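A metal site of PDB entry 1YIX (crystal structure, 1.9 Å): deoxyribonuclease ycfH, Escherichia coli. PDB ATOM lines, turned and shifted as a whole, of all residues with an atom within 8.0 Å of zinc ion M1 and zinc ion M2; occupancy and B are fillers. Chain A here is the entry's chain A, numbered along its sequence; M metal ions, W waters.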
ATOM      1  N   HIS A   7      -7.418  -7.561   7.495  1.00  0.00           N
ATOM      2  CA  HIS A   7      -6.369  -6.873   6.756  1.00  0.00           C
ATOM      3  C   HIS A   7      -5.413  -7.838   6.054  1.00  0.00           C
ATOM      4  O   HIS A   7      -4.521  -8.440   6.690  1.00  0.00           O
ATOM      5  CB  HIS A   7      -5.589  -6.017   7.744  1.00  0.00           C
ATOM      6  CG  HIS A   7      -4.641  -5.071   7.088  1.00  0.00           C
ATOM      7  ND1 HIS A   7      -4.923  -3.723   6.949  1.00  0.00           N
ATOM      8  CD2 HIS A   7      -3.423  -5.267   6.527  1.00  0.00           C
ATOM      9  CE1 HIS A   7      -3.913  -3.139   6.322  1.00  0.00           C
ATOM     10  NE2 HIS A   7      -2.995  -4.053   6.056  1.00  0.00           N
ATOM     11  N   CYS A   8      -5.599  -7.999   4.743  1.00  0.00           N
ATOM     12  CA  CYS A   8      -4.738  -8.870   3.945  1.00  0.00           C
ATOM     13  C   CYS A   8      -4.462  -8.287   2.569  1.00  0.00           C
ATOM     14  O   CYS A   8      -5.316  -7.609   1.973  1.00  0.00           O
ATOM     15  CB  CYS A   8      -5.350 -10.278   3.842  1.00  0.00           C
ATOM     16  SG  CYS A   8      -6.969 -10.353   3.029  1.00  0.00           S
ATOM     17  N   HIS A   9      -3.254  -8.533   2.063  1.00  0.00           N
ATOM     18  CA  HIS A   9      -2.875  -8.007   0.757  1.00  0.00           C
ATOM     19  C   HIS A   9      -3.044  -9.146  -0.250  1.00  0.00           C
ATOM     20  O   HIS A   9      -2.067  -9.826  -0.609  1.00  0.00           O
ATOM     21  CB  HIS A   9      -1.428  -7.478   0.797  1.00  0.00           C
ATOM     22  CG  HIS A   9      -1.237  -6.271   1.661  1.00  0.00           C
ATOM     23  ND1 HIS A   9      -1.542  -4.997   1.231  1.00  0.00           N
ATOM     24  CD2 HIS A   9      -0.862  -6.142   2.954  1.00  0.00           C
ATOM     25  CE1 HIS A   9      -1.366  -4.135   2.230  1.00  0.00           C
ATOM     26  NE2 HIS A   9      -0.952  -4.813   3.285  1.00  0.00           N
ATOM     27  N   VAL A  40      -6.742  -5.183   1.012  1.00  0.00           N
ATOM     28  CA  VAL A  40      -6.019  -3.912   1.067  1.00  0.00           C
ATOM     29  C   VAL A  40      -5.096  -3.577  -0.105  1.00  0.00           C
ATOM     30  O   VAL A  40      -4.184  -4.338  -0.418  1.00  0.00           O
ATOM     31  CB  VAL A  40      -5.127  -3.870   2.366  1.00  0.00           C
ATOM     32  CG1 VAL A  40      -4.439  -2.508   2.503  1.00  0.00           C
ATOM     33  CG2 VAL A  40      -5.962  -4.192   3.587  1.00  0.00           C
ATOM     34  N   ALA A  41      -5.299  -2.422  -0.735  1.00  0.00           N
ATOM     35  CA  ALA A  41      -4.454  -1.971  -1.850  1.00  0.00           C
ATOM     36  C   ALA A  41      -3.452  -0.973  -1.258  1.00  0.00           C
ATOM     37  O   ALA A  41      -3.779  -0.325  -0.259  1.00  0.00           O
ATOM     38  CB  ALA A  41      -5.309  -1.302  -2.908  1.00  0.00           C
ATOM     39  N   THR A  42      -2.273  -0.859  -1.864  1.00  0.00           N
ATOM     40  CA  THR A  42      -1.210   0.056  -1.398  1.00  0.00           C
ATOM     41  C   THR A  42      -1.053   1.350  -2.211  1.00  0.00           C
ATOM     42  O   THR A  42      -0.335   2.270  -1.772  1.00  0.00           O
ATOM     43  CB  THR A  42       0.180  -0.618  -1.384  1.00  0.00           C
ATOM     44  OG1 THR A  42       0.510  -1.058  -2.693  1.00  0.00           O
ATOM     45  CG2 THR A  42       0.204  -1.802  -0.450  1.00  0.00           C
ATOM     46  N   HIS A  67      -0.659   3.810   0.722  1.00  0.00           N
ATOM     47  CA  HIS A  67       0.219   3.456   1.841  1.00  0.00           C
ATOM     48  C   HIS A  67       1.273   4.526   2.167  1.00  0.00           C
ATOM     49  O   HIS A  67       1.767   5.213   1.283  1.00  0.00           O
ATOM     50  CB  HIS A  67       0.917   2.151   1.453  1.00  0.00           C
ATOM     51  CG  HIS A  67       1.657   1.480   2.569  1.00  0.00           C
ATOM     52  ND1 HIS A  67       1.234   0.281   3.116  1.00  0.00           N
ATOM     53  CD2 HIS A  67       2.836   1.776   3.159  1.00  0.00           C
ATOM     54  CE1 HIS A  67       2.134  -0.134   3.993  1.00  0.00           C
ATOM     55  NE2 HIS A  67       3.111   0.759   4.042  1.00  0.00           N
ATOM     56  N   PRO A  68       1.649   4.653   3.446  1.00  0.00           N
ATOM     57  CA  PRO A  68       2.655   5.611   3.914  1.00  0.00           C
ATOM     58  C   PRO A  68       3.986   5.450   3.219  1.00  0.00           C
ATOM     59  O   PRO A  68       4.704   6.428   2.989  1.00  0.00           O
ATOM     60  CB  PRO A  68       2.771   5.280   5.399  1.00  0.00           C
ATOM     61  CG  PRO A  68       1.378   4.945   5.763  1.00  0.00           C
ATOM     62  CD  PRO A  68       0.934   4.066   4.590  1.00  0.00           C
ATOM     63  N   LEU A  69       4.322   4.211   2.868  1.00  0.00           N
ATOM     64  CA  LEU A  69       5.592   3.958   2.227  1.00  0.00           C
ATOM     65  C   LEU A  69       5.560   4.140   0.710  1.00  0.00           C
ATOM     66  O   LEU A  69       6.599   4.048   0.044  1.00  0.00           O
ATOM     67  CB  LEU A  69       6.070   2.555   2.600  1.00  0.00           C
ATOM     68  CG  LEU A  69       6.443   2.403   4.083  1.00  0.00           C
ATOM     69  CD1 LEU A  69       7.143   1.047   4.293  1.00  0.00           C
ATOM     70  CD2 LEU A  69       7.381   3.533   4.503  1.00  0.00           C
ATOM     71  N   GLU A  94      -4.714   1.423   3.176  1.00  0.00           N
ATOM     72  CA  GLU A  94      -4.161   1.793   4.467  1.00  0.00           C
ATOM     73  C   GLU A  94      -3.347   3.085   4.354  1.00  0.00           C
ATOM     74  O   GLU A  94      -2.608   3.315   3.388  1.00  0.00           O
ATOM     75  CB  GLU A  94      -3.323   0.650   5.076  1.00  0.00           C
ATOM     76  CG  GLU A  94      -2.055   0.309   4.332  1.00  0.00           C
ATOM     77  CD  GLU A  94      -1.309  -0.806   5.032  1.00  0.00           C
ATOM     78  OE1 GLU A  94      -1.417  -1.949   4.580  1.00  0.00           O
ATOM     79  OE2 GLU A  94      -0.657  -0.523   6.047  1.00  0.00           O
ATOM     80  N   THR A  95      -3.549   3.945   5.341  1.00  0.00           N
ATOM     81  CA  THR A  95      -2.870   5.226   5.388  1.00  0.00           C
ATOM     82  C   THR A  95      -2.067   5.216   6.694  1.00  0.00           C
ATOM     83  O   THR A  95      -1.796   4.142   7.243  1.00  0.00           O
ATOM     84  CB  THR A  95      -3.922   6.404   5.331  1.00  0.00           C
ATOM     85  OG1 THR A  95      -3.241   7.664   5.302  1.00  0.00           O
ATOM     86  CG2 THR A  95      -4.883   6.356   6.512  1.00  0.00           C
ATOM     87  N   ASP A  98       4.864   5.968   8.464  1.00  0.00           N
ATOM     88  CA  ASP A  98       5.906   4.991   8.667  1.00  0.00           C
ATOM     89  C   ASP A  98       7.236   5.729   8.519  1.00  0.00           C
ATOM     90  O   ASP A  98       7.607   6.134   7.413  1.00  0.00           O
ATOM     91  CB  ASP A  98       5.793   3.866   7.636  1.00  0.00           C
ATOM     92  CG  ASP A  98       6.667   2.701   7.956  1.00  0.00           C
ATOM     93  OD1 ASP A  98       6.220   1.555   7.763  1.00  0.00           O
ATOM     94  OD2 ASP A  98       7.808   2.939   8.425  1.00  0.00           O
ATOM     95  N   ILE A 128      -7.982   2.842   7.757  1.00  0.00           N
ATOM     96  CA  ILE A 128      -7.169   1.717   8.243  1.00  0.00           C
ATOM     97  C   ILE A 128      -5.814   2.382   8.396  1.00  0.00           C
ATOM     98  O   ILE A 128      -5.231   2.842   7.424  1.00  0.00           O
ATOM     99  CB  ILE A 128      -7.094   0.591   7.211  1.00  0.00           C
ATOM    100  CG1 ILE A 128      -8.476  -0.056   7.078  1.00  0.00           C
ATOM    101  CG2 ILE A 128      -6.096  -0.467   7.667  1.00  0.00           C
ATOM    102  CD1 ILE A 128      -8.599  -1.028   5.907  1.00  0.00           C
ATOM    103  N   VAL A 129      -5.338   2.451   9.637  1.00  0.00           N
ATOM    104  CA  VAL A 129      -4.107   3.148   9.965  1.00  0.00           C
ATOM    105  C   VAL A 129      -2.951   2.230  10.246  1.00  0.00           C
ATOM    106  O   VAL A 129      -3.030   1.375  11.133  1.00  0.00           O
ATOM    107  CB  VAL A 129      -4.289   4.061  11.216  1.00  0.00           C
ATOM    108  CG1 VAL A 129      -2.990   4.844  11.504  1.00  0.00           C
ATOM    109  CG2 VAL A 129      -5.492   5.068  10.996  1.00  0.00           C
ATOM    110  N   HIS A 130      -1.885   2.458   9.491  1.00  0.00           N
ATOM    111  CA  HIS A 130      -0.618   1.765   9.616  1.00  0.00           C
ATOM    112  C   HIS A 130       0.275   2.813  10.274  1.00  0.00           C
ATOM    113  O   HIS A 130       0.331   3.944   9.802  1.00  0.00           O
ATOM    114  CB  HIS A 130      -0.033   1.476   8.223  1.00  0.00           C
ATOM    115  CG  HIS A 130       1.421   1.099   8.237  1.00  0.00           C
ATOM    116  ND1 HIS A 130       1.858  -0.207   8.157  1.00  0.00           N
ATOM    117  CD2 HIS A 130       2.535   1.864   8.336  1.00  0.00           C
ATOM    118  CE1 HIS A 130       3.171  -0.229   8.207  1.00  0.00           C
ATOM    119  NE2 HIS A 130       3.614   1.007   8.318  1.00  0.00           N
ATOM    120  N   THR A 131       0.960   2.468  11.358  1.00  0.00           N
ATOM    121  CA  THR A 131       1.877   3.405  11.993  1.00  0.00           C
ATOM    122  C   THR A 131       3.107   2.602  12.424  1.00  0.00           C
ATOM    123  O   THR A 131       2.992   1.420  12.753  1.00  0.00           O
ATOM    124  CB  THR A 131       1.240   4.129  13.249  1.00  0.00           C
ATOM    125  OG1 THR A 131       2.046   5.257  13.613  1.00  0.00           O
ATOM    126  CG2 THR A 131       1.177   3.195  14.467  1.00  0.00           C
ATOM    127  N   HIS A 155      -4.413  -0.853  12.503  1.00  0.00           N
ATOM    128  CA  HIS A 155      -4.137  -2.195  11.965  1.00  0.00           C
ATOM    129  C   HIS A 155      -2.730  -2.706  12.330  1.00  0.00           C
ATOM    130  O   HIS A 155      -1.800  -1.919  12.421  1.00  0.00           O
ATOM    131  CB  HIS A 155      -4.377  -2.200  10.436  1.00  0.00           C
ATOM    132  CG  HIS A 155      -3.134  -2.382   9.623  1.00  0.00           C
ATOM    133  ND1 HIS A 155      -2.601  -3.617   9.356  1.00  0.00           N
ATOM    134  CD2 HIS A 155      -2.254  -1.479   9.123  1.00  0.00           C
ATOM    135  CE1 HIS A 155      -1.445  -3.485   8.733  1.00  0.00           C
ATOM    136  NE2 HIS A 155      -1.206  -2.191   8.582  1.00  0.00           N
ATOM    137  N   CYS A 156      -2.590  -4.026  12.503  1.00  0.00           N
ATOM    138  CA  CYS A 156      -1.293  -4.632  12.838  1.00  0.00           C
ATOM    139  C   CYS A 156      -0.563  -3.877  13.960  1.00  0.00           C
ATOM    140  O   CYS A 156       0.611  -3.504  13.835  1.00  0.00           O
ATOM    141  CB  CYS A 156      -0.423  -4.694  11.579  1.00  0.00           C
ATOM    142  SG  CYS A 156       1.091  -5.726  11.715  1.00  0.00           S
ATOM    143  N   GLU A 203      -6.128  -9.917  12.265  1.00  0.00           N
ATOM    144  CA  GLU A 203      -5.772  -9.922  10.853  1.00  0.00           C
ATOM    145  C   GLU A 203      -4.501 -10.702  10.696  1.00  0.00           C
ATOM    146  O   GLU A 203      -3.872 -11.076  11.677  1.00  0.00           O
ATOM    147  CB  GLU A 203      -5.473  -8.519  10.410  1.00  0.00           C
ATOM    148  CG  GLU A 203      -4.193  -7.997  11.086  1.00  0.00           C
ATOM    149  CD  GLU A 203      -3.954  -6.532  10.850  1.00  0.00           C
ATOM    150  OE1 GLU A 203      -4.671  -5.700  11.467  1.00  0.00           O
ATOM    151  OE2 GLU A 203      -3.057  -6.214  10.043  1.00  0.00           O
ATOM    152  N   THR A 204      -4.085 -10.877   9.447  1.00  0.00           N
ATOM    153  CA  THR A 204      -2.820 -11.547   9.127  1.00  0.00           C
ATOM    154  C   THR A 204      -1.824 -10.542   8.521  1.00  0.00           C
ATOM    155  O   THR A 204      -0.641 -10.644   8.746  1.00  0.00           O
ATOM    156  CB  THR A 204      -3.011 -12.671   8.075  1.00  0.00           C
ATOM    157  OG1 THR A 204      -3.643 -12.128   6.888  1.00  0.00           O
ATOM    158  CG2 THR A 204      -3.882 -13.795   8.638  1.00  0.00           C
ATOM    159  N   ASP A 205      -2.323  -9.532   7.797  1.00  0.00           N
ATOM    160  CA  ASP A 205      -1.483  -8.598   7.030  1.00  0.00           C
ATOM    161  C   ASP A 205      -0.708  -9.486   6.014  1.00  0.00           C
ATOM    162  O   ASP A 205       0.451  -9.213   5.681  1.00  0.00           O
ATOM    163  CB  ASP A 205      -0.495  -7.795   7.895  1.00  0.00           C
ATOM    164  CG  ASP A 205      -0.026  -6.502   7.194  1.00  0.00           C
ATOM    165  OD1 ASP A 205      -0.553  -6.209   6.086  1.00  0.00           O
ATOM    166  OD2 ASP A 205       0.852  -5.782   7.749  1.00  0.00           O
ATOM    167  N   SER A 206      -1.376 -10.533   5.547  1.00  0.00           N
ATOM    168  CA  SER A 206      -0.799 -11.457   4.558  1.00  0.00           C
ATOM    169  C   SER A 206      -0.289 -10.670   3.362  1.00  0.00           C
ATOM    170  O   SER A 206      -0.943  -9.722   2.924  1.00  0.00           O
ATOM    171  CB  SER A 206      -1.836 -12.467   4.068  1.00  0.00           C
ATOM    172  OG  SER A 206      -2.160 -13.433   5.042  1.00  0.00           O
ATOM    173  N   PRO A 207       0.819 -11.125   2.768  1.00  0.00           N
ATOM    174  CA  PRO A 207       1.602 -12.332   3.087  1.00  0.00           C
ATOM    175  C   PRO A 207       2.693 -12.258   4.175  1.00  0.00           C
ATOM    176  O   PRO A 207       3.458 -13.215   4.363  1.00  0.00           O
ATOM    177  CB  PRO A 207       2.203 -12.689   1.730  1.00  0.00           C
ATOM    178  CG  PRO A 207       2.592 -11.329   1.214  1.00  0.00           C
ATOM    179  CD  PRO A 207       1.331 -10.490   1.527  1.00  0.00           C
ATOM    180  N   TYR A 208       2.758 -11.147   4.894  1.00  0.00           N
ATOM    181  CA  TYR A 208       3.773 -10.983   5.922  1.00  0.00           C
ATOM    182  C   TYR A 208       3.375 -11.492   7.304  1.00  0.00           C
ATOM    183  O   TYR A 208       2.211 -11.778   7.574  1.00  0.00           O
ATOM    184  CB  TYR A 208       4.142  -9.508   6.097  1.00  0.00           C
ATOM    185  CG  TYR A 208       4.098  -8.714   4.826  1.00  0.00           C
ATOM    186  CD1 TYR A 208       4.921  -9.046   3.749  1.00  0.00           C
ATOM    187  CD2 TYR A 208       3.169  -7.682   4.657  1.00  0.00           C
ATOM    188  CE1 TYR A 208       4.823  -8.378   2.543  1.00  0.00           C
ATOM    189  CE2 TYR A 208       3.051  -7.005   3.458  1.00  0.00           C
ATOM    190  CZ  TYR A 208       3.880  -7.359   2.398  1.00  0.00           C
ATOM    191  OH  TYR A 208       3.751  -6.710   1.202  1.00  0.00           O
ATOM    192  N   LEU A 209       4.372 -11.592   8.171  1.00  0.00           N
ATOM    193  CA  LEU A 209       4.146 -11.939   9.568  1.00  0.00           C
ATOM    194  C   LEU A 209       3.341 -13.179   9.923  1.00  0.00           C
ATOM    195  O   LEU A 209       2.425 -13.111  10.754  1.00  0.00           O
ATOM    196  CB  LEU A 209       3.507 -10.729  10.238  1.00  0.00           C
ATOM    197  CG  LEU A 209       4.209  -9.425   9.868  1.00  0.00           C
ATOM    198  CD1 LEU A 209       3.481  -8.245  10.493  1.00  0.00           C
ATOM    199  CD2 LEU A 209       5.665  -9.493  10.358  1.00  0.00           C
HETATM  200 ZN    ZN M   1       0.376  -1.780   7.310  1.00  0.00          ZN
HETATM  201 ZN    ZN M   2      -1.041  -4.009   5.182  1.00  0.00          ZN
HETATM  202  O   HOH W   1       1.896  -3.211   8.748  1.00  0.00           O
HETATM  203  O   HOH W   2       2.550  -2.785   4.924  1.00  0.00           O
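The backbone NH of His 67 sits close to the backbone carbonyl oxygen of Glu 94, at 3.3 Å. A ring nitrogen (NE2) of His 130 is in hydrogen-bond range of the side-chain carboxylate (OD1) of Asp 98. A ring nitrogen (ND1) of His 9 sits at hydrogen-bond distance from the backbone carbonyl oxygen of Val 40. N of His 130 sits at hydrogen-bond distance from O of Thr 95 (2.8 Å). The backbone NH of His 155 lies within hydrogen-bond range of the backbone carbonyl oxygen of Val 129 (3.0 Å). ND1 of His 7 sits close to ND1 of His 155 (3.3 Å). ND1 of His 155 lies within hydrogen-bond range of OE2 of Glu 203 (2.7 Å). The backbone carbonyl oxygen (O) of Ser 206 is in hydrogen-bond range of the backbone NH (N) of His 9 (2.7 Å).
The nearest printed residue that does not touch zinc ion M1 is Asp 205 (4.1 Å).
Five residues have an atom within 4 Å of zinc ion M2: His 7, His 9, Glu 94, His 155 and Asp 205. The nearest printed residue that does not touch zinc ion M2 is Val 40 (4.6 Å).
Zinc ion M1 is bound by OE2 of Glu 94 (2.1 Å), NE2 of His 155 (2.1 Å), ND1 of His 130 (2.3 Å) and water W1 (2.5 Å). Zinc ion M1 has four donor atoms within binding distance.
Zinc ion M2 is bound by NE2 of His 9, NE2 of His 7, OE1 of Glu 94 and OD1 of Asp 205.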
